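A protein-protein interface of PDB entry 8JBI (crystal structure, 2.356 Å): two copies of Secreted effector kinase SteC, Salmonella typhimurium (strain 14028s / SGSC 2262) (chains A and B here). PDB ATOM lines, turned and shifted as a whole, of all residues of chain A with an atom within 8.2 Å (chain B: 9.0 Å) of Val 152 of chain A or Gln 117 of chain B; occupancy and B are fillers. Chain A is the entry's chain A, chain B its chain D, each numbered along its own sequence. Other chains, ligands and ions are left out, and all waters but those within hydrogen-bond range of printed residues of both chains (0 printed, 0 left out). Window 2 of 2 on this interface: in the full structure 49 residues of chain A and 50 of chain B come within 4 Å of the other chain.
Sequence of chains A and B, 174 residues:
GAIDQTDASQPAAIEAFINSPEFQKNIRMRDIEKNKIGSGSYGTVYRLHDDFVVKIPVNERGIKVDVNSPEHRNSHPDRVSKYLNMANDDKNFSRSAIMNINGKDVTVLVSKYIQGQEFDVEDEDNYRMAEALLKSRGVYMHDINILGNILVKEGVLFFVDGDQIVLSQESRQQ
No position is printed for both chains. Of the 11 pairs that touch across the chains among the printed residues, none has its exchanged pair printed and touching as well.
The backbone carbonyl oxygen (O) of Leu 151 of chain A is in hydrogen-bond range of the backbone NH (N) of Phe 158 of chain A (2.8 Å).
O of Ile 150 of chain A touches CA of Glu 118 of chain B, at 3.8 Å. Ile 114 of chain B touches Leu 151 of chain A. O of Gln 117 of chain B touches CA of Leu 151 of chain A (3.4 Å). Gly 116 of chain B touches Val 152 of chain A (CA to O, 3.5 Å). CD1 of Phe 119 of chain B touches CG1 of Val 152 of chain A (3.7 Å). Gln 115 of chain B touches Lys 153 of chain A. Leu 157 of chain A touches Phe 119 of chain B (CD2 to CD1, 3.7 Å). Met 129 of chain B touches Leu 157 of chain A. Phe 158 of chain A touches Ile 114 of chain B.
Printed residues of chain A that touch a printed residue of chain B: Ile 150, Leu 151, Val 152, Lys 153, Leu 157 and Phe 158. Of the 10 printed residues of chain B, 7 touch a printed residue of chain A. Printed residues of chain B that touch a printed residue of chain A: Ile 114, Gln 115, Gly 116, Gln 117, Glu 118, Phe 119 and Met 129. Hydrophobic or aromatic side chains of chain B that line the printed part of chain A: Ile 114, Phe 119 and Met 129. Among the printed residues, 11 pairs touch across the chains. Among the printed residues, no Asp or Glu carboxylate lies within 4 Å of a Lys or Arg side-chain nitrogen of the other chain.
Val 152 of chain A touches just these residues of chain B: Gly 116, Gln 117 and Phe 119. Glu 154 of chain A touches none of the printed residues of chain B. Printed residues of chain B within 4 Å of Leu 157 of chain A: Phe 119 (3.7 Å) and Met 129 (3.8 Å). Of the printed residues of chain B, Phe 158 of chain A touches Ile 114. Tyr 113 of chain B touches none of the printed residues of chain A. Gln 117 of chain B touches two residues of chain A. Of the printed residues of chain A, Glu 118 of chain B touches Ile 150. The nearest residue of chain A that does not touch Gln 117 of chain B is Ile 150 of chain A (4.3 Å).
The backbone carbonyl oxygen of Gln 117 of chain B sits at hydrogen-bond distance from the backbone NH of Val 152 of chain A (3.1 Å). N of Phe 119 of chain B sits at hydrogen-bond distance from O of Ile 150 of chain A (3.0 Å).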
ATOM      1  N   ASN A 149     -13.294 -22.325  21.560  1.00  0.00           N
ATOM      2  CA  ASN A 149     -14.009 -22.664  20.329  1.00  0.00           C
ATOM      3  C   ASN A 149     -13.556 -24.029  19.790  1.00  0.00           C
ATOM      4  O   ASN A 149     -12.462 -24.506  20.111  1.00  0.00           O
ATOM      5  CB  ASN A 149     -13.832 -21.567  19.260  1.00  0.00           C
ATOM      6  CG  ASN A 149     -14.509 -20.225  19.638  1.00  0.00           C
ATOM      7  OD1 ASN A 149     -15.390 -20.167  20.503  1.00  0.00           O
ATOM      8  ND2 ASN A 149     -14.087 -19.145  18.975  1.00  0.00           N
ATOM      9  N   ILE A 150     -14.389 -24.671  18.980  1.00  0.00           N
ATOM     10  CA  ILE A 150     -14.004 -25.958  18.400  1.00  0.00           C
ATOM     11  C   ILE A 150     -13.724 -25.831  16.906  1.00  0.00           C
ATOM     12  O   ILE A 150     -14.555 -25.311  16.156  1.00  0.00           O
ATOM     13  CB  ILE A 150     -15.069 -27.043  18.640  1.00  0.00           C
ATOM     14  CG1 ILE A 150     -15.544 -26.996  20.094  1.00  0.00           C
ATOM     15  CG2 ILE A 150     -14.507 -28.440  18.297  1.00  0.00           C
ATOM     16  CD1 ILE A 150     -16.532 -28.072  20.457  1.00  0.00           C
ATOM     17  N   LEU A 151     -12.542 -26.286  16.490  1.00  0.00           N
ATOM     18  CA  LEU A 151     -12.178 -26.354  15.071  1.00  0.00           C
ATOM     19  C   LEU A 151     -11.937 -27.800  14.663  1.00  0.00           C
ATOM     20  O   LEU A 151     -11.455 -28.617  15.459  1.00  0.00           O
ATOM     21  CB  LEU A 151     -10.919 -25.537  14.793  1.00  0.00           C
ATOM     22  CG  LEU A 151     -10.949 -24.079  15.244  1.00  0.00           C
ATOM     23  CD1 LEU A 151      -9.580 -23.451  15.046  1.00  0.00           C
ATOM     24  CD2 LEU A 151     -12.011 -23.300  14.482  1.00  0.00           C
ATOM     25  N   VAL A 152     -12.283 -28.125  13.424  1.00  0.00           N
ATOM     26  CA  VAL A 152     -12.025 -29.465  12.914  1.00  0.00           C
ATOM     27  C   VAL A 152     -11.141 -29.405  11.669  1.00  0.00           C
ATOM     28  O   VAL A 152     -11.394 -28.639  10.737  1.00  0.00           O
ATOM     29  CB  VAL A 152     -13.334 -30.262  12.659  1.00  0.00           C
ATOM     30  CG1 VAL A 152     -14.307 -29.458  11.793  1.00  0.00           C
ATOM     31  CG2 VAL A 152     -13.021 -31.643  12.049  1.00  0.00           C
ATOM     32  N   LYS A 153     -10.081 -30.193  11.679  1.00  0.00           N
ATOM     33  CA  LYS A 153      -9.142 -30.187  10.578  1.00  0.00           C
ATOM     34  C   LYS A 153      -8.957 -31.620  10.128  1.00  0.00           C
ATOM     35  O   LYS A 153      -8.420 -32.436  10.880  1.00  0.00           O
ATOM     36  CB  LYS A 153      -7.806 -29.588  11.015  1.00  0.00           C
ATOM     37  CG  LYS A 153      -6.861 -29.303   9.858  1.00  0.00           C
ATOM     38  CD  LYS A 153      -5.574 -28.635  10.332  1.00  0.00           C
ATOM     39  CE  LYS A 153      -4.581 -29.649  10.872  1.00  0.00           C
ATOM     40  NZ  LYS A 153      -3.311 -29.019  11.346  1.00  0.00           N
ATOM     41  N   GLU A 154      -9.436 -31.921   8.922  1.00  0.00           N
ATOM     42  CA  GLU A 154      -9.321 -33.259   8.349  1.00  0.00           C
ATOM     43  C   GLU A 154      -9.841 -34.316   9.313  1.00  0.00           C
ATOM     44  O   GLU A 154      -9.154 -35.335   9.553  1.00  0.00           O
ATOM     45  CB  GLU A 154      -7.860 -33.566   8.009  1.00  0.00           C
ATOM     46  CG  GLU A 154      -7.279 -32.674   6.915  1.00  0.00           C
ATOM     47  CD  GLU A 154      -5.824 -33.007   6.584  1.00  0.00           C
ATOM     48  OE1 GLU A 154      -5.419 -32.773   5.421  1.00  0.00           O
ATOM     49  OE2 GLU A 154      -5.091 -33.487   7.485  1.00  0.00           O
ATOM     50  N   GLY A 155     -11.021 -34.060   9.887  1.00  0.00           N
ATOM     51  CA  GLY A 155     -11.646 -34.994  10.808  1.00  0.00           C
ATOM     52  C   GLY A 155     -11.154 -34.933  12.255  1.00  0.00           C
ATOM     53  O   GLY A 155     -11.721 -35.595  13.129  1.00  0.00           O
ATOM     54  N   VAL A 156     -10.122 -34.134  12.520  1.00  0.00           N
ATOM     55  CA  VAL A 156      -9.554 -34.039  13.866  1.00  0.00           C
ATOM     56  C   VAL A 156      -9.935 -32.745  14.615  1.00  0.00           C
ATOM     57  O   VAL A 156      -9.771 -31.639  14.097  1.00  0.00           O
ATOM     58  CB  VAL A 156      -8.025 -34.197  13.820  1.00  0.00           C
ATOM     59  CG1 VAL A 156      -7.428 -34.112  15.222  1.00  0.00           C
ATOM     60  CG2 VAL A 156      -7.664 -35.520  13.172  1.00  0.00           C
ATOM     61  N   LEU A 157     -10.420 -32.898  15.846  1.00  0.00           N
ATOM     62  CA  LEU A 157     -10.880 -31.765  16.668  1.00  0.00           C
ATOM     63  C   LEU A 157      -9.760 -31.051  17.416  1.00  0.00           C
ATOM     64  O   LEU A 157      -8.901 -31.690  18.039  1.00  0.00           O
ATOM     65  CB  LEU A 157     -11.934 -32.216  17.692  1.00  0.00           C
ATOM     66  CG  LEU A 157     -13.244 -32.793  17.161  1.00  0.00           C
ATOM     67  CD1 LEU A 157     -14.268 -32.936  18.278  1.00  0.00           C
ATOM     68  CD2 LEU A 157     -13.787 -31.925  16.049  1.00  0.00           C
ATOM     69  N   PHE A 158      -9.788 -29.725  17.359  1.00  0.00           N
ATOM     70  CA  PHE A 158      -8.866 -28.889  18.112  1.00  0.00           C
ATOM     71  C   PHE A 158      -9.614 -27.827  18.910  1.00  0.00           C
ATOM     72  O   PHE A 158     -10.695 -27.371  18.528  1.00  0.00           O
ATOM     73  CB  PHE A 158      -7.864 -28.227  17.173  1.00  0.00           C
ATOM     74  CG  PHE A 158      -6.925 -29.196  16.537  1.00  0.00           C
ATOM     75  CD1 PHE A 158      -7.265 -29.840  15.353  1.00  0.00           C
ATOM     76  CD2 PHE A 158      -5.711 -29.486  17.132  1.00  0.00           C
ATOM     77  CE1 PHE A 158      -6.397 -30.754  14.778  1.00  0.00           C
ATOM     78  CE2 PHE A 158      -4.843 -30.394  16.549  1.00  0.00           C
ATOM     79  CZ  PHE A 158      -5.192 -31.027  15.381  1.00  0.00           C
ATOM     80  N   PHE A 159      -9.014 -27.422  20.014  1.00  0.00           N
ATOM     81  CA  PHE A 159      -9.684 -26.545  20.958  1.00  0.00           C
ATOM     82  C   PHE A 159      -8.858 -25.283  21.120  1.00  0.00           C
ATOM     83  O   PHE A 159      -7.701 -25.341  21.527  1.00  0.00           O
ATOM     84  CB  PHE A 159      -9.878 -27.306  22.266  1.00  0.00           C
ATOM     85  CG  PHE A 159     -10.733 -28.531  22.096  1.00  0.00           C
ATOM     86  CD1 PHE A 159     -12.115 -28.415  22.013  1.00  0.00           C
ATOM     87  CD2 PHE A 159     -10.159 -29.788  21.951  1.00  0.00           C
ATOM     88  CE1 PHE A 159     -12.929 -29.543  21.814  1.00  0.00           C
ATOM     89  CE2 PHE A 159     -10.956 -30.923  21.761  1.00  0.00           C
ATOM     90  CZ  PHE A 159     -12.349 -30.797  21.681  1.00  0.00           C
ATOM     91  N   TYR B 113      -1.248 -22.576  15.273  1.00  0.00           N
ATOM     92  CA  TYR B 113      -2.248 -22.095  14.323  1.00  0.00           C
ATOM     93  C   TYR B 113      -2.988 -23.299  13.770  1.00  0.00           C
ATOM     94  O   TYR B 113      -2.366 -24.261  13.335  1.00  0.00           O
ATOM     95  CB  TYR B 113      -1.610 -21.295  13.187  1.00  0.00           C
ATOM     96  CG  TYR B 113      -2.577 -21.006  12.064  1.00  0.00           C
ATOM     97  CD1 TYR B 113      -3.644 -20.128  12.248  1.00  0.00           C
ATOM     98  CD2 TYR B 113      -2.433 -21.614  10.822  1.00  0.00           C
ATOM     99  CE1 TYR B 113      -4.539 -19.863  11.232  1.00  0.00           C
ATOM    100  CE2 TYR B 113      -3.330 -21.359   9.791  1.00  0.00           C
ATOM    101  CZ  TYR B 113      -4.377 -20.482  10.004  1.00  0.00           C
ATOM    102  OH  TYR B 113      -5.262 -20.227   8.983  1.00  0.00           O
ATOM    103  N   ILE B 114      -4.313 -23.270  13.835  1.00  0.00           N
ATOM    104  CA  ILE B 114      -5.102 -24.371  13.305  1.00  0.00           C
ATOM    105  C   ILE B 114      -5.934 -23.890  12.138  1.00  0.00           C
ATOM    106  O   ILE B 114      -6.868 -23.098  12.312  1.00  0.00           O
ATOM    107  CB  ILE B 114      -6.061 -24.981  14.342  1.00  0.00           C
ATOM    108  CG1 ILE B 114      -5.316 -25.407  15.613  1.00  0.00           C
ATOM    109  CG2 ILE B 114      -6.801 -26.158  13.723  1.00  0.00           C
ATOM    110  CD1 ILE B 114      -4.314 -26.560  15.413  1.00  0.00           C
ATOM    111  N   GLN B 115      -5.597 -24.368  10.943  1.00  0.00           N
ATOM    112  CA  GLN B 115      -6.389 -24.041   9.773  1.00  0.00           C
ATOM    113  C   GLN B 115      -7.494 -25.077   9.642  1.00  0.00           C
ATOM    114  O   GLN B 115      -7.241 -26.222   9.279  1.00  0.00           O
ATOM    115  CB  GLN B 115      -5.518 -24.023   8.516  1.00  0.00           C
ATOM    116  CG  GLN B 115      -6.047 -23.109   7.414  1.00  0.00           C
ATOM    117  CD  GLN B 115      -5.303 -23.280   6.099  1.00  0.00           C
ATOM    118  OE1 GLN B 115      -4.342 -24.051   6.009  1.00  0.00           O
ATOM    119  NE2 GLN B 115      -5.748 -22.564   5.066  1.00  0.00           N
ATOM    120  N   GLY B 116      -8.719 -24.680   9.958  1.00  0.00           N
ATOM    121  CA  GLY B 116      -9.841 -25.589   9.859  1.00  0.00           C
ATOM    122  C   GLY B 116     -11.151 -24.833   9.831  1.00  0.00           C
ATOM    123  O   GLY B 116     -11.176 -23.602   9.895  1.00  0.00           O
ATOM    124  N   GLN B 117     -12.247 -25.572   9.735  1.00  0.00           N
ATOM    125  CA  GLN B 117     -13.566 -24.966   9.752  1.00  0.00           C
ATOM    126  C   GLN B 117     -14.122 -25.007  11.165  1.00  0.00           C
ATOM    127  O   GLN B 117     -13.615 -25.745  12.019  1.00  0.00           O
ATOM    128  CB  GLN B 117     -14.492 -25.712   8.798  1.00  0.00           C
ATOM    129  CG  GLN B 117     -14.421 -27.219   8.937  1.00  0.00           C
ATOM    130  CD  GLN B 117     -14.412 -27.928   7.590  1.00  0.00           C
ATOM    131  OE1 GLN B 117     -15.158 -27.559   6.681  1.00  0.00           O
ATOM    132  NE2 GLN B 117     -13.556 -28.946   7.455  1.00  0.00           N
ATOM    133  N   GLU B 118     -15.155 -24.212  11.423  1.00  0.00           N
ATOM    134  CA  GLU B 118     -15.812 -24.287  12.712  1.00  0.00           C
ATOM    135  C   GLU B 118     -16.538 -25.617  12.824  1.00  0.00           C
ATOM    136  O   GLU B 118     -17.275 -26.012  11.908  1.00  0.00           O
ATOM    137  CB  GLU B 118     -16.805 -23.142  12.912  1.00  0.00           C
ATOM    138  CG  GLU B 118     -17.473 -23.188  14.284  1.00  0.00           C
ATOM    139  CD  GLU B 118     -17.592 -21.823  14.937  1.00  0.00           C
ATOM    140  OE1 GLU B 118     -16.932 -21.596  15.981  1.00  0.00           O
ATOM    141  OE2 GLU B 118     -18.358 -20.985  14.411  1.00  0.00           O
ATOM    142  N   PHE B 119     -16.304 -26.316  13.932  1.00  0.00           N
ATOM    143  CA  PHE B 119     -17.054 -27.525  14.236  1.00  0.00           C
ATOM    144  C   PHE B 119     -18.352 -27.121  14.944  1.00  0.00           C
ATOM    145  O   PHE B 119     -18.330 -26.535  16.027  1.00  0.00           O
ATOM    146  CB  PHE B 119     -16.220 -28.446  15.109  1.00  0.00           C
ATOM    147  CG  PHE B 119     -16.789 -29.827  15.260  1.00  0.00           C
ATOM    148  CD1 PHE B 119     -16.796 -30.708  14.187  1.00  0.00           C
ATOM    149  CD2 PHE B 119     -17.280 -30.262  16.488  1.00  0.00           C
ATOM    150  CE1 PHE B 119     -17.306 -32.000  14.320  1.00  0.00           C
ATOM    151  CE2 PHE B 119     -17.785 -31.549  16.636  1.00  0.00           C
ATOM    152  CZ  PHE B 119     -17.792 -32.423  15.547  1.00  0.00           C
ATOM    153  N   ASP B 120     -19.473 -27.425  14.303  1.00  0.00           N
ATOM    154  CA  ASP B 120     -20.795 -27.055  14.779  1.00  0.00           C
ATOM    155  C   ASP B 120     -21.313 -28.050  15.807  1.00  0.00           C
ATOM    156  O   ASP B 120     -21.597 -29.193  15.469  1.00  0.00           O
ATOM    157  CB  ASP B 120     -21.766 -27.007  13.591  1.00  0.00           C
ATOM    158  CG  ASP B 120     -23.175 -26.607  13.997  1.00  0.00           C
ATOM    159  OD1 ASP B 120     -23.315 -25.834  14.966  1.00  0.00           O
ATOM    160  OD2 ASP B 120     -24.140 -27.058  13.335  1.00  0.00           O
ATOM    161  N   ASN B 126     -22.501 -34.182  16.723  1.00  0.00           N
ATOM    162  CA  ASN B 126     -21.226 -33.497  16.882  1.00  0.00           C
ATOM    163  C   ASN B 126     -20.903 -33.137  18.325  1.00  0.00           C
ATOM    164  O   ASN B 126     -19.752 -33.234  18.754  1.00  0.00           O
ATOM    165  CB  ASN B 126     -21.211 -32.223  16.049  1.00  0.00           C
ATOM    166  CG  ASN B 126     -20.987 -32.488  14.584  1.00  0.00           C
ATOM    167  OD1 ASN B 126     -20.891 -33.634  14.159  1.00  0.00           O
ATOM    168  ND2 ASN B 126     -20.905 -31.420  13.799  1.00  0.00           N
ATOM    169  N   MET B 129     -19.910 -36.191  20.182  1.00  0.00           N
ATOM    170  CA  MET B 129     -18.577 -36.612  19.749  1.00  0.00           C
ATOM    171  C   MET B 129     -17.481 -35.774  20.396  1.00  0.00           C
ATOM    172  O   MET B 129     -16.492 -36.327  20.867  1.00  0.00           O
ATOM    173  CB  MET B 129     -18.446 -36.593  18.221  1.00  0.00           C
ATOM    174  CG  MET B 129     -17.235 -37.379  17.714  1.00  0.00           C
ATOM    175  SD  MET B 129     -15.811 -36.307  17.404  1.00  0.00           S
ATOM    176  CE  MET B 129     -16.201 -35.867  15.681  1.00  0.00           C
